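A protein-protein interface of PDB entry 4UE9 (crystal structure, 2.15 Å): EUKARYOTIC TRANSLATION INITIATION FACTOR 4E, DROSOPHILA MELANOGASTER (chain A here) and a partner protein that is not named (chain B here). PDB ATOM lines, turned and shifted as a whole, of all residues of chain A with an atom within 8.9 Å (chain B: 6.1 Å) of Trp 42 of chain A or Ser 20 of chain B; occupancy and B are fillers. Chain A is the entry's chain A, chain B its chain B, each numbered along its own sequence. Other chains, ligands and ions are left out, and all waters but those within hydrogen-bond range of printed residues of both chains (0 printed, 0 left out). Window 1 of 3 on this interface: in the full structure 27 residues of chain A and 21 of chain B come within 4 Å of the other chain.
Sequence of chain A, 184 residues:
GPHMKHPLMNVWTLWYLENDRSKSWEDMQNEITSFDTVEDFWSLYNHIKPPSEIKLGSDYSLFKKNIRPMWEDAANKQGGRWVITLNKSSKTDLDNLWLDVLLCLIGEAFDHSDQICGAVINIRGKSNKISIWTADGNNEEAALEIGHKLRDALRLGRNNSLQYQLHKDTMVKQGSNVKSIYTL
The indole nitrogen (NE1) of Trp 42 of chain A is in hydrogen-bond range of the backbone carbonyl oxygen (O) of Leu 11 of chain B, 2.8 Å away. N of Ser 43 of chain A sits close to O of Ser 20 of chain B (3.4 Å). The side-chain hydroxyl (OG) of Ser 43 of chain A lies within hydrogen-bond range of the backbone carbonyl oxygen (O) of Gln 25 of chain B (2.9 Å). The backbone carbonyl oxygen of Ser 20 of chain B is in hydrogen-bond range of the side-chain amide nitrogen of Asn 46 of chain A (2.9 Å).
Of the 13 printed residues of chain B, 8 touch a printed residue of chain A. Hydrophobic or aromatic side chains of chain B that line the printed part of chain A: Leu 11, Leu 12 and Leu 14. Among the printed residues, 20 pairs touch across the chains. Among the printed residues, no Asp or Glu carboxylate lies within 4 Å of a Lys or Arg side-chain nitrogen of the other chain.
NZ of Lys 5 of chain A is in salt-bridge range of OD1 of Asp 40 of chain A (3.0 Å). The backbone NH (N) of Val 38 of chain A sits at hydrogen-bond distance from the backbone carbonyl oxygen (O) of His 6 of chain A, 2.8 Å away. OE2 of Glu 39 of chain A sits at hydrogen-bond distance from ND1 of His 6 of chain A. A ring nitrogen (ND1) of His 47 of chain A sits at hydrogen-bond distance from the backbone carbonyl oxygen (O) of Ser 43 of chain A, at 2.8 Å. The backbone carbonyl oxygen of Leu 14 of chain B sits at hydrogen-bond distance from the side-chain hydroxyl of Ser 20 of chain B, at 2.9 Å. The backbone carbonyl oxygen of Gly 18 of chain B sits at hydrogen-bond distance from the backbone NH of Gln 25 of chain B.
Of chain B, only Leu 11, Leu 12, Leu 14, Arg 15 and Ser 20 come within 4 Å of Trp 42 of chain A. Of the printed residues of chain B, Ser 43 of chain A touches Lys 19, Ser 20 and Gln 25. Of the printed residues of chain B, His 47 of chain A touches Arg 21 and Gln 25. Of the printed residues of chain B, Leu 103 of chain A touches Leu 11 (3.3 Å) and Leu 12 (3.9 Å). Of the printed residues of chain A, Leu 12 of chain B touches Trp 42 (3.6 Å) and Leu 103 (3.9 Å). Of chain A, only Trp 42 (3.4 Å), Tyr 45 (3.7 Å) and Asn 46 (3.5 Å) come within 4 Å of Arg 15 of chain B. No residue of chain A comes within 4 Å of Gly 18 of chain B. Of the printed residues of chain A, Ser 20 of chain B touches Glu 39, Trp 42, Ser 43 and Asn 46. Arg 21 of chain B touches just one residue of chain A: His 47. The nearest printed residue of chain B that does not touch His 47 of chain A is Ser 20 of chain B (5.0 Å).
Among the printed residues, pairs that only touch across the chains: Leu 103 of chain A with Leu 11 of chain B (3.3 Å), His 6 of chain A with Leu 14 of chain B (3.3 Å), Glu 39 of chain A with Ser 20 of chain B (3.4 Å), Trp 42 of chain A with Arg 15 of chain B (3.4 Å), Asn 46 of chain A with Arg 15 of chain B (3.5 Å), Lys 5 of chain A with Lys 19 of chain B (3.5 Å), His 47 of chain A with Arg 21 of chain B (3.5 Å), Ser 43 of chain A with Lys 19 of chain B (3.6 Å), Trp 42 of chain A with Leu 14 of chain B (3.6 Å), Trp 42 of chain A with Leu 12 of chain B (3.6 Å), Trp 42 of chain A with Ser 20 of chain B (3.7 Å), Tyr 45 of chain A with Arg 15 of chain B (3.7 Å), His 47 of chain A with Gln 25 of chain B (3.7 Å), Val 38 of chain A with Leu 14 of chain B (3.8 Å), Val 38 of chain A with Leu 11 of chain B (3.9 Å) and Leu 103 of chain A with Leu 12 of chain B (3.9 Å).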
ATOM      1  N   LYS A   5      34.745  24.307  -3.646  1.00  0.00           N
ATOM      2  CA  LYS A   5      33.334  24.049  -3.902  1.00  0.00           C
ATOM      3  C   LYS A   5      32.486  25.284  -3.614  1.00  0.00           C
ATOM      4  O   LYS A   5      32.867  26.138  -2.810  1.00  0.00           O
ATOM      5  CB  LYS A   5      32.839  22.875  -3.056  1.00  0.00           C
ATOM      6  CG  LYS A   5      33.471  21.539  -3.404  1.00  0.00           C
ATOM      7  CD  LYS A   5      32.922  20.428  -2.519  1.00  0.00           C
ATOM      8  CE  LYS A   5      33.496  19.074  -2.897  1.00  0.00           C
ATOM      9  NZ  LYS A   5      32.928  17.975  -2.067  1.00  0.00           N
ATOM     10  N   HIS A   6      31.336  25.370  -4.276  1.00  0.00           N
ATOM     11  CA  HIS A   6      30.392  26.460  -4.055  1.00  0.00           C
ATOM     12  C   HIS A   6      29.278  25.996  -3.120  1.00  0.00           C
ATOM     13  O   HIS A   6      28.519  25.092  -3.471  1.00  0.00           O
ATOM     14  CB  HIS A   6      29.802  26.943  -5.382  1.00  0.00           C
ATOM     15  CG  HIS A   6      30.822  27.494  -6.328  1.00  0.00           C
ATOM     16  ND1 HIS A   6      31.664  26.690  -7.067  1.00  0.00           N
ATOM     17  CD2 HIS A   6      31.137  28.770  -6.653  1.00  0.00           C
ATOM     18  CE1 HIS A   6      32.451  27.447  -7.808  1.00  0.00           C
ATOM     19  NE2 HIS A   6      32.154  28.713  -7.576  1.00  0.00           N
ATOM     20  N   LEU A   8      25.805  25.648  -0.964  1.00  0.00           N
ATOM     21  CA  LEU A   8      24.386  25.942  -1.108  1.00  0.00           C
ATOM     22  C   LEU A   8      23.865  26.555   0.182  1.00  0.00           C
ATOM     23  O   LEU A   8      24.426  26.324   1.254  1.00  0.00           O
ATOM     24  CB  LEU A   8      23.599  24.675  -1.448  1.00  0.00           C
ATOM     25  CG  LEU A   8      24.013  23.940  -2.724  1.00  0.00           C
ATOM     26  CD1 LEU A   8      23.237  22.643  -2.863  1.00  0.00           C
ATOM     27  CD2 LEU A   8      23.806  24.820  -3.945  1.00  0.00           C
ATOM     28  N   PHE A  35      23.619  16.622   0.270  1.00  0.00           N
ATOM     29  CA  PHE A  35      24.659  17.472  -0.295  1.00  0.00           C
ATOM     30  C   PHE A  35      24.400  18.928   0.065  1.00  0.00           C
ATOM     31  O   PHE A  35      23.257  19.316   0.314  1.00  0.00           O
ATOM     32  CB  PHE A  35      24.725  17.306  -1.816  1.00  0.00           C
ATOM     33  CG  PHE A  35      23.452  17.674  -2.524  1.00  0.00           C
ATOM     34  CD1 PHE A  35      23.213  18.982  -2.920  1.00  0.00           C
ATOM     35  CD2 PHE A  35      22.492  16.713  -2.795  1.00  0.00           C
ATOM     36  CE1 PHE A  35      22.041  19.322  -3.568  1.00  0.00           C
ATOM     37  CE2 PHE A  35      21.318  17.048  -3.446  1.00  0.00           C
ATOM     38  CZ  PHE A  35      21.094  18.354  -3.833  1.00  0.00           C
ATOM     39  N   THR A  37      26.668  21.507  -1.549  1.00  0.00           N
ATOM     40  CA  THR A  37      27.444  22.285  -2.509  1.00  0.00           C
ATOM     41  C   THR A  37      26.933  22.028  -3.922  1.00  0.00           C
ATOM     42  O   THR A  37      26.306  21.001  -4.185  1.00  0.00           O
ATOM     43  CB  THR A  37      28.947  21.946  -2.450  1.00  0.00           C
ATOM     44  OG1 THR A  37      29.160  20.618  -2.944  1.00  0.00           O
ATOM     45  CG2 THR A  37      29.478  22.059  -1.022  1.00  0.00           C
ATOM     46  N   VAL A  38      27.203  22.966  -4.825  1.00  0.00           N
ATOM     47  CA  VAL A  38      26.772  22.849  -6.213  1.00  0.00           C
ATOM     48  C   VAL A  38      27.485  21.688  -6.895  1.00  0.00           C
ATOM     49  O   VAL A  38      26.885  20.961  -7.686  1.00  0.00           O
ATOM     50  CB  VAL A  38      27.043  24.149  -7.005  1.00  0.00           C
ATOM     51  CG1 VAL A  38      26.563  24.019  -8.449  1.00  0.00           C
ATOM     52  CG2 VAL A  38      26.367  25.335  -6.331  1.00  0.00           C
ATOM     53  N   GLU A  39      28.767  21.520  -6.583  1.00  0.00           N
ATOM     54  CA  GLU A  39      29.571  20.466  -7.190  1.00  0.00           C
ATOM     55  C   GLU A  39      29.028  19.087  -6.833  1.00  0.00           C
ATOM     56  O   GLU A  39      28.899  18.218  -7.695  1.00  0.00           O
ATOM     57  CB  GLU A  39      31.035  20.578  -6.752  1.00  0.00           C
ATOM     58  CG  GLU A  39      31.809  21.711  -7.414  1.00  0.00           C
ATOM     59  CD  GLU A  39      31.421  23.083  -6.897  1.00  0.00           C
ATOM     60  OE1 GLU A  39      30.623  23.163  -5.939  1.00  0.00           O
ATOM     61  OE2 GLU A  39      31.919  24.086  -7.450  1.00  0.00           O
ATOM     62  N   ASP A  40      28.709  18.895  -5.556  1.00  0.00           N
ATOM     63  CA  ASP A  40      28.221  17.608  -5.071  1.00  0.00           C
ATOM     64  C   ASP A  40      26.820  17.302  -5.604  1.00  0.00           C
ATOM     65  O   ASP A  40      26.452  16.139  -5.763  1.00  0.00           O
ATOM     66  CB  ASP A  40      28.222  17.582  -3.540  1.00  0.00           C
ATOM     67  CG  ASP A  40      29.629  17.616  -2.954  1.00  0.00           C
ATOM     68  OD1 ASP A  40      30.541  17.001  -3.544  1.00  0.00           O
ATOM     69  OD2 ASP A  40      29.822  18.256  -1.897  1.00  0.00           O
ATOM     70  N   PHE A  41      26.036  18.341  -5.875  1.00  0.00           N
ATOM     71  CA  PHE A  41      24.736  18.147  -6.508  1.00  0.00           C
ATOM     72  C   PHE A  41      24.903  17.500  -7.877  1.00  0.00           C
ATOM     73  O   PHE A  41      24.257  16.501  -8.189  1.00  0.00           O
ATOM     74  CB  PHE A  41      23.989  19.472  -6.657  1.00  0.00           C
ATOM     75  CG  PHE A  41      22.870  19.421  -7.661  1.00  0.00           C
ATOM     76  CD1 PHE A  41      21.652  18.848  -7.332  1.00  0.00           C
ATOM     77  CD2 PHE A  41      23.041  19.936  -8.936  1.00  0.00           C
ATOM     78  CE1 PHE A  41      20.619  18.799  -8.256  1.00  0.00           C
ATOM     79  CE2 PHE A  41      22.012  19.891  -9.863  1.00  0.00           C
ATOM     80  CZ  PHE A  41      20.801  19.322  -9.522  1.00  0.00           C
ATOM     81  N   TRP A  42      25.774  18.085  -8.692  1.00  0.00           N
ATOM     82  CA  TRP A  42      26.013  17.586 -10.039  1.00  0.00           C
ATOM     83  C   TRP A  42      26.652  16.204 -10.015  1.00  0.00           C
ATOM     84  O   TRP A  42      26.332  15.354 -10.844  1.00  0.00           O
ATOM     85  CB  TRP A  42      26.900  18.555 -10.819  1.00  0.00           C
ATOM     86  CG  TRP A  42      26.202  19.817 -11.201  1.00  0.00           C
ATOM     87  CD1 TRP A  42      26.518  21.083 -10.805  1.00  0.00           C
ATOM     88  CD2 TRP A  42      25.060  19.936 -12.055  1.00  0.00           C
ATOM     89  NE1 TRP A  42      25.646  21.986 -11.366  1.00  0.00           N
ATOM     90  CE2 TRP A  42      24.738  21.305 -12.137  1.00  0.00           C
ATOM     91  CE3 TRP A  42      24.277  19.017 -12.760  1.00  0.00           C
ATOM     92  CZ2 TRP A  42      23.670  21.778 -12.895  1.00  0.00           C
ATOM     93  CZ3 TRP A  42      23.218  19.486 -13.511  1.00  0.00           C
ATOM     94  CH2 TRP A  42      22.923  20.854 -13.574  1.00  0.00           C
ATOM     95  N   SER A  43      27.557  15.986  -9.066  1.00  0.00           N
ATOM     96  CA  SER A  43      28.206  14.688  -8.916  1.00  0.00           C
ATOM     97  C   SER A  43      27.159  13.601  -8.703  1.00  0.00           C
ATOM     98  O   SER A  43      27.308  12.475  -9.177  1.00  0.00           O
ATOM     99  CB  SER A  43      29.195  14.711  -7.748  1.00  0.00           C
ATOM    100  OG  SER A  43      29.841  13.458  -7.603  1.00  0.00           O
ATOM    101  N   LEU A  44      26.094  13.954  -7.991  1.00  0.00           N
ATOM    102  CA  LEU A  44      24.989  13.038  -7.754  1.00  0.00           C
ATOM    103  C   LEU A  44      24.085  12.946  -8.979  1.00  0.00           C
ATOM    104  O   LEU A  44      23.723  11.854  -9.414  1.00  0.00           O
ATOM    105  CB  LEU A  44      24.182  13.488  -6.534  1.00  0.00           C
ATOM    106  CG  LEU A  44      22.869  12.750  -6.265  1.00  0.00           C
ATOM    107  CD1 LEU A  44      23.104  11.254  -6.102  1.00  0.00           C
ATOM    108  CD2 LEU A  44      22.195  13.326  -5.035  1.00  0.00           C
ATOM    109  N   TYR A  45      23.728  14.100  -9.535  1.00  0.00           N
ATOM    110  CA  TYR A  45      22.800  14.152 -10.661  1.00  0.00           C
ATOM    111  C   TYR A  45      23.394  13.511 -11.913  1.00  0.00           C
ATOM    112  O   TYR A  45      22.670  12.928 -12.719  1.00  0.00           O
ATOM    113  CB  TYR A  45      22.401  15.599 -10.961  1.00  0.00           C
ATOM    114  CG  TYR A  45      21.342  15.723 -12.037  1.00  0.00           C
ATOM    115  CD1 TYR A  45      19.991  15.646 -11.721  1.00  0.00           C
ATOM    116  CD2 TYR A  45      21.693  15.910 -13.367  1.00  0.00           C
ATOM    117  CE1 TYR A  45      19.020  15.753 -12.701  1.00  0.00           C
ATOM    118  CE2 TYR A  45      20.731  16.017 -14.353  1.00  0.00           C
ATOM    119  CZ  TYR A  45      19.397  15.940 -14.015  1.00  0.00           C
ATOM    120  OH  TYR A  45      18.437  16.049 -14.997  1.00  0.00           O
ATOM    121  N   ASN A  46      24.709  13.619 -12.073  1.00  0.00           N
ATOM    122  CA  ASN A  46      25.378  13.077 -13.252  1.00  0.00           C
ATOM    123  C   ASN A  46      25.449  11.553 -13.251  1.00  0.00           C
ATOM    124  O   ASN A  46      25.746  10.944 -14.278  1.00  0.00           O
ATOM    125  CB  ASN A  46      26.797  13.643 -13.370  1.00  0.00           C
ATOM    126  CG  ASN A  46      26.817  15.107 -13.775  1.00  0.00           C
ATOM    127  OD1 ASN A  46      25.909  15.595 -14.448  1.00  0.00           O
ATOM    128  ND2 ASN A  46      27.865  15.816 -13.367  1.00  0.00           N
ATOM    129  N   HIS A  47      25.174  10.939 -12.101  1.00  0.00           N
ATOM    130  CA  HIS A  47      25.325   9.493 -11.947  1.00  0.00           C
ATOM    131  C   HIS A  47      24.018   8.783 -11.590  1.00  0.00           C
ATOM    132  O   HIS A  47      24.033   7.619 -11.187  1.00  0.00           O
ATOM    133  CB  HIS A  47      26.386   9.195 -10.885  1.00  0.00           C
ATOM    134  CG  HIS A  47      27.780   9.522 -11.324  1.00  0.00           C
ATOM    135  ND1 HIS A  47      28.313  10.788 -11.227  1.00  0.00           N
ATOM    136  CD2 HIS A  47      28.744   8.747 -11.875  1.00  0.00           C
ATOM    137  CE1 HIS A  47      29.550  10.779 -11.695  1.00  0.00           C
ATOM    138  NE2 HIS A  47      29.835   9.554 -12.093  1.00  0.00           N
ATOM    139  N   ILE A  48      22.896   9.482 -11.743  1.00  0.00           N
ATOM    140  CA  ILE A  48      21.579   8.871 -11.571  1.00  0.00           C
ATOM    141  C   ILE A  48      20.767   9.008 -12.857  1.00  0.00           C
ATOM    142  O   ILE A  48      20.971   9.941 -13.633  1.00  0.00           O
ATOM    143  CB  ILE A  48      20.798   9.499 -10.396  1.00  0.00           C
ATOM    144  CG1 ILE A  48      20.558  10.996 -10.635  1.00  0.00           C
ATOM    145  CG2 ILE A  48      21.546   9.268  -9.093  1.00  0.00           C
ATOM    146  CD1 ILE A  48      19.634  11.644  -9.614  1.00  0.00           C
ATOM    147  N   ASN A  96      14.398  17.930 -18.598  1.00  0.00           N
ATOM    148  CA  ASN A  96      14.874  19.297 -18.423  1.00  0.00           C
ATOM    149  C   ASN A  96      13.970  20.105 -17.503  1.00  0.00           C
ATOM    150  O   ASN A  96      14.414  21.060 -16.864  1.00  0.00           O
ATOM    151  CB  ASN A  96      14.989  19.998 -19.776  1.00  0.00           C
ATOM    152  CG  ASN A  96      16.137  19.467 -20.609  1.00  0.00           C
ATOM    153  OD1 ASN A  96      17.284  19.457 -20.167  1.00  0.00           O
ATOM    154  ND2 ASN A  96      15.832  19.012 -21.818  1.00  0.00           N
ATOM    155  N   LEU A  99      14.905  19.043 -13.867  1.00  0.00           N
ATOM    156  CA  LEU A  99      16.179  19.655 -13.513  1.00  0.00           C
ATOM    157  C   LEU A  99      16.011  21.139 -13.184  1.00  0.00           C
ATOM    158  O   LEU A  99      16.565  21.628 -12.202  1.00  0.00           O
ATOM    159  CB  LEU A  99      17.187  19.479 -14.651  1.00  0.00           C
ATOM    160  CG  LEU A  99      18.553  20.143 -14.459  1.00  0.00           C
ATOM    161  CD1 LEU A  99      19.207  19.711 -13.152  1.00  0.00           C
ATOM    162  CD2 LEU A  99      19.459  19.826 -15.635  1.00  0.00           C
ATOM    163  N   ASP A 100      15.241  21.851 -14.002  1.00  0.00           N
ATOM    164  CA  ASP A 100      14.995  23.270 -13.765  1.00  0.00           C
ATOM    165  C   ASP A 100      14.307  23.488 -12.421  1.00  0.00           C
ATOM    166  O   ASP A 100      14.545  24.491 -11.750  1.00  0.00           O
ATOM    167  CB  ASP A 100      14.154  23.866 -14.893  1.00  0.00           C
ATOM    168  CG  ASP A 100      14.965  24.130 -16.148  1.00  0.00           C
ATOM    169  OD1 ASP A 100      16.096  23.608 -16.252  1.00  0.00           O
ATOM    170  OD2 ASP A 100      14.471  24.857 -17.032  1.00  0.00           O
ATOM    171  N   LEU A 102      14.817  21.505  -9.848  1.00  0.00           N
ATOM    172  CA  LEU A 102      15.876  21.264  -8.876  1.00  0.00           C
ATOM    173  C   LEU A 102      16.775  22.488  -8.748  1.00  0.00           C
ATOM    174  O   LEU A 102      17.139  22.885  -7.641  1.00  0.00           O
ATOM    175  CB  LEU A 102      16.707  20.039  -9.268  1.00  0.00           C
ATOM    176  CG  LEU A 102      15.986  18.688  -9.299  1.00  0.00           C
ATOM    177  CD1 LEU A 102      16.980  17.562  -9.541  1.00  0.00           C
ATOM    178  CD2 LEU A 102      15.201  18.437  -8.023  1.00  0.00           C
ATOM    179  N   LEU A 103      17.126  23.090  -9.881  1.00  0.00           N
ATOM    180  CA  LEU A 103      17.980  24.271  -9.882  1.00  0.00           C
ATOM    181  C   LEU A 103      17.290  25.441  -9.187  1.00  0.00           C
ATOM    182  O   LEU A 103      17.938  26.235  -8.507  1.00  0.00           O
ATOM    183  CB  LEU A 103      18.365  24.655 -11.313  1.00  0.00           C
ATOM    184  CG  LEU A 103      19.188  23.625 -12.092  1.00  0.00           C
ATOM    185  CD1 LEU A 103      19.475  24.127 -13.499  1.00  0.00           C
ATOM    186  CD2 LEU A 103      20.486  23.288 -11.374  1.00  0.00           C
ATOM    187  N   ILE A 106      17.686  24.464  -5.149  1.00  0.00           N
ATOM    188  CA  ILE A 106      19.005  24.588  -4.537  1.00  0.00           C
ATOM    189  C   ILE A 106      19.598  25.973  -4.790  1.00  0.00           C
ATOM    190  O   ILE A 106      20.413  26.460  -4.007  1.00  0.00           O
ATOM    191  CB  ILE A 106      19.971  23.492  -5.050  1.00  0.00           C
ATOM    192  CG1 ILE A 106      20.298  23.683  -6.536  1.00  0.00           C
ATOM    193  CG2 ILE A 106      19.362  22.111  -4.810  1.00  0.00           C
ATOM    194  CD1 ILE A 106      21.398  22.771  -7.044  1.00  0.00           C
ATOM    195  N   ASP B  10      24.387  30.167 -13.313  1.00  0.00           N
ATOM    196  CA  ASP B  10      25.477  29.938 -12.372  1.00  0.00           C
ATOM    197  C   ASP B  10      25.587  28.461 -12.018  1.00  0.00           C
ATOM    198  O   ASP B  10      26.685  27.919 -11.914  1.00  0.00           O
ATOM    199  CB  ASP B  10      25.276  30.766 -11.100  1.00  0.00           C
ATOM    200  CG  ASP B  10      25.353  32.260 -11.355  1.00  0.00           C
ATOM    201  OD1 ASP B  10      26.038  32.670 -12.316  1.00  0.00           O
ATOM    202  OD2 ASP B  10      24.729  33.024 -10.589  1.00  0.00           O
ATOM    203  N   LEU B  11      24.439  27.814 -11.843  1.00  0.00           N
ATOM    204  CA  LEU B  11      24.404  26.408 -11.464  1.00  0.00           C
ATOM    205  C   LEU B  11      24.865  25.508 -12.607  1.00  0.00           C
ATOM    206  O   LEU B  11      25.698  24.622 -12.411  1.00  0.00           O
ATOM    207  CB  LEU B  11      22.994  26.019 -11.018  1.00  0.00           C
ATOM    208  CG  LEU B  11      22.507  26.692  -9.731  1.00  0.00           C
ATOM    209  CD1 LEU B  11      21.033  26.412  -9.500  1.00  0.00           C
ATOM    210  CD2 LEU B  11      23.329  26.234  -8.530  1.00  0.00           C
ATOM    211  N   LEU B  12      24.324  25.737 -13.799  1.00  0.00           N
ATOM    212  CA  LEU B  12      24.696  24.950 -14.969  1.00  0.00           C
ATOM    213  C   LEU B  12      26.162  25.159 -15.338  1.00  0.00           C
ATOM    214  O   LEU B  12      26.813  24.256 -15.864  1.00  0.00           O
ATOM    215  CB  LEU B  12      23.805  25.307 -16.161  1.00  0.00           C
ATOM    216  CG  LEU B  12      22.352  24.832 -16.089  1.00  0.00           C
ATOM    217  CD1 LEU B  12      21.535  25.453 -17.212  1.00  0.00           C
ATOM    218  CD2 LEU B  12      22.276  23.316 -16.154  1.00  0.00           C
ATOM    219  N   ALA B  13      26.673  26.354 -15.058  1.00  0.00           N
ATOM    220  CA  ALA B  13      28.054  26.696 -15.385  1.00  0.00           C
ATOM    221  C   ALA B  13      29.049  25.809 -14.638  1.00  0.00           C
ATOM    222  O   ALA B  13      30.175  25.612 -15.093  1.00  0.00           O
ATOM    223  CB  ALA B  13      28.319  28.161 -15.074  1.00  0.00           C
ATOM    224  N   LEU B  14      28.629  25.278 -13.493  1.00  0.00           N
ATOM    225  CA  LEU B  14      29.499  24.446 -12.663  1.00  0.00           C
ATOM    226  C   LEU B  14      29.226  22.956 -12.856  1.00  0.00           C
ATOM    227  O   LEU B  14      29.693  22.129 -12.075  1.00  0.00           O
ATOM    228  CB  LEU B  14      29.325  24.810 -11.186  1.00  0.00           C
ATOM    229  CG  LEU B  14      29.721  26.232 -10.785  1.00  0.00           C
ATOM    230  CD1 LEU B  14      29.294  26.515  -9.356  1.00  0.00           C
ATOM    231  CD2 LEU B  14      31.219  26.444 -10.946  1.00  0.00           C
ATOM    232  N   ARG B  15      28.477  22.612 -13.898  1.00  0.00           N
ATOM    233  CA  ARG B  15      28.044  21.233 -14.088  1.00  0.00           C
ATOM    234  C   ARG B  15      29.194  20.285 -14.420  1.00  0.00           C
ATOM    235  O   ARG B  15      29.126  19.097 -14.104  1.00  0.00           O
ATOM    236  CB  ARG B  15      26.985  21.147 -15.191  1.00  0.00           C
ATOM    237  CG  ARG B  15      26.504  19.724 -15.436  1.00  0.00           C
ATOM    238  CD  ARG B  15      25.250  19.666 -16.287  1.00  0.00           C
ATOM    239  NE  ARG B  15      24.702  18.313 -16.320  1.00  0.00           N
ATOM    240  CZ  ARG B  15      23.641  17.947 -17.034  1.00  0.00           C
ATOM    241  NH1 ARG B  15      23.003  18.831 -17.787  1.00  0.00           N
ATOM    242  NH2 ARG B  15      23.220  16.690 -16.997  1.00  0.00           N
ATOM    243  N   TYR B  16      30.244  20.806 -15.049  1.00  0.00           N
ATOM    244  CA  TYR B  16      31.334  19.966 -15.536  1.00  0.00           C
ATOM    245  C   TYR B  16      32.673  20.281 -14.872  1.00  0.00           C
ATOM    246  O   TYR B  16      33.731  20.142 -15.487  1.00  0.00           O
ATOM    247  CB  TYR B  16      31.456  20.106 -17.054  1.00  0.00           C
ATOM    248  CG  TYR B  16      30.234  19.606 -17.787  1.00  0.00           C
ATOM    249  CD1 TYR B  16      30.023  18.245 -17.973  1.00  0.00           C
ATOM    250  CD2 TYR B  16      29.286  20.489 -18.286  1.00  0.00           C
ATOM    251  CE1 TYR B  16      28.905  17.780 -18.637  1.00  0.00           C
ATOM    252  CE2 TYR B  16      28.165  20.033 -18.953  1.00  0.00           C
ATOM    253  CZ  TYR B  16      27.979  18.677 -19.125  1.00  0.00           C
ATOM    254  OH  TYR B  16      26.865  18.219 -19.789  1.00  0.00           O
ATOM    255  N   GLU B  17      32.624  20.693 -13.609  1.00  0.00           N
ATOM    256  CA  GLU B  17      33.838  20.865 -12.823  1.00  0.00           C
ATOM    257  C   GLU B  17      34.450  19.500 -12.535  1.00  0.00           C
ATOM    258  O   GLU B  17      33.818  18.468 -12.763  1.00  0.00           O
ATOM    259  CB  GLU B  17      33.545  21.603 -11.514  1.00  0.00           C
ATOM    260  CG  GLU B  17      32.951  22.990 -11.694  1.00  0.00           C
ATOM    261  CD  GLU B  17      33.880  23.939 -12.425  1.00  0.00           C
ATOM    262  OE1 GLU B  17      34.289  23.619 -13.562  1.00  0.00           O
ATOM    263  OE2 GLU B  17      34.196  25.010 -11.867  1.00  0.00           O
ATOM    264  N   GLY B  18      35.681  19.497 -12.033  1.00  0.00           N
ATOM    265  CA  GLY B  18      36.372  18.259 -11.724  1.00  0.00           C
ATOM    266  C   GLY B  18      35.644  17.447 -10.669  1.00  0.00           C
ATOM    267  O   GLY B  18      35.547  16.223 -10.771  1.00  0.00           O
ATOM    268  N   LYS B  19      35.128  18.133  -9.655  1.00  0.00           N
ATOM    269  CA  LYS B  19      34.420  17.475  -8.563  1.00  0.00           C
ATOM    270  C   LYS B  19      32.980  17.152  -8.948  1.00  0.00           C
ATOM    271  O   LYS B  19      32.349  16.282  -8.347  1.00  0.00           O
ATOM    272  CB  LYS B  19      34.450  18.353  -7.311  1.00  0.00           C
ATOM    273  CG  LYS B  19      35.856  18.656  -6.815  1.00  0.00           C
ATOM    274  CD  LYS B  19      35.837  19.445  -5.516  1.00  0.00           C
ATOM    275  CE  LYS B  19      37.245  19.728  -5.016  1.00  0.00           C
ATOM    276  NZ  LYS B  19      37.244  20.462  -3.718  1.00  0.00           N
ATOM    277  N   SER B  20      32.467  17.857  -9.952  1.00  0.00           N
ATOM    278  CA  SER B  20      31.110  17.633 -10.440  1.00  0.00           C
ATOM    279  C   SER B  20      31.048  16.417 -11.357  1.00  0.00           C
ATOM    280  O   SER B  20      30.011  15.761 -11.465  1.00  0.00           O
ATOM    281  CB  SER B  20      30.599  18.868 -11.183  1.00  0.00           C
ATOM    282  OG  SER B  20      30.623  20.011 -10.348  1.00  0.00           O
ATOM    283  N   ARG B  21      32.163  16.127 -12.021  1.00  0.00           N
ATOM    284  CA  ARG B  21      32.243  14.996 -12.940  1.00  0.00           C
ATOM    285  C   ARG B  21      32.647  13.725 -12.202  1.00  0.00           C
ATOM    286  O   ARG B  21      32.407  12.615 -12.679  1.00  0.00           O
ATOM    287  CB  ARG B  21      33.240  15.291 -14.064  1.00  0.00           C
ATOM    288  N   GLN B  25      34.447  13.306  -9.720  1.00  0.00           N
ATOM    289  CA  GLN B  25      34.195  11.897  -9.444  1.00  0.00           C
ATOM    290  C   GLN B  25      32.708  11.643  -9.230  1.00  0.00           C
ATOM    291  O   GLN B  25      31.885  12.545  -9.394  1.00  0.00           O
ATOM    292  CB  GLN B  25      34.987  11.443  -8.217  1.00  0.00           C
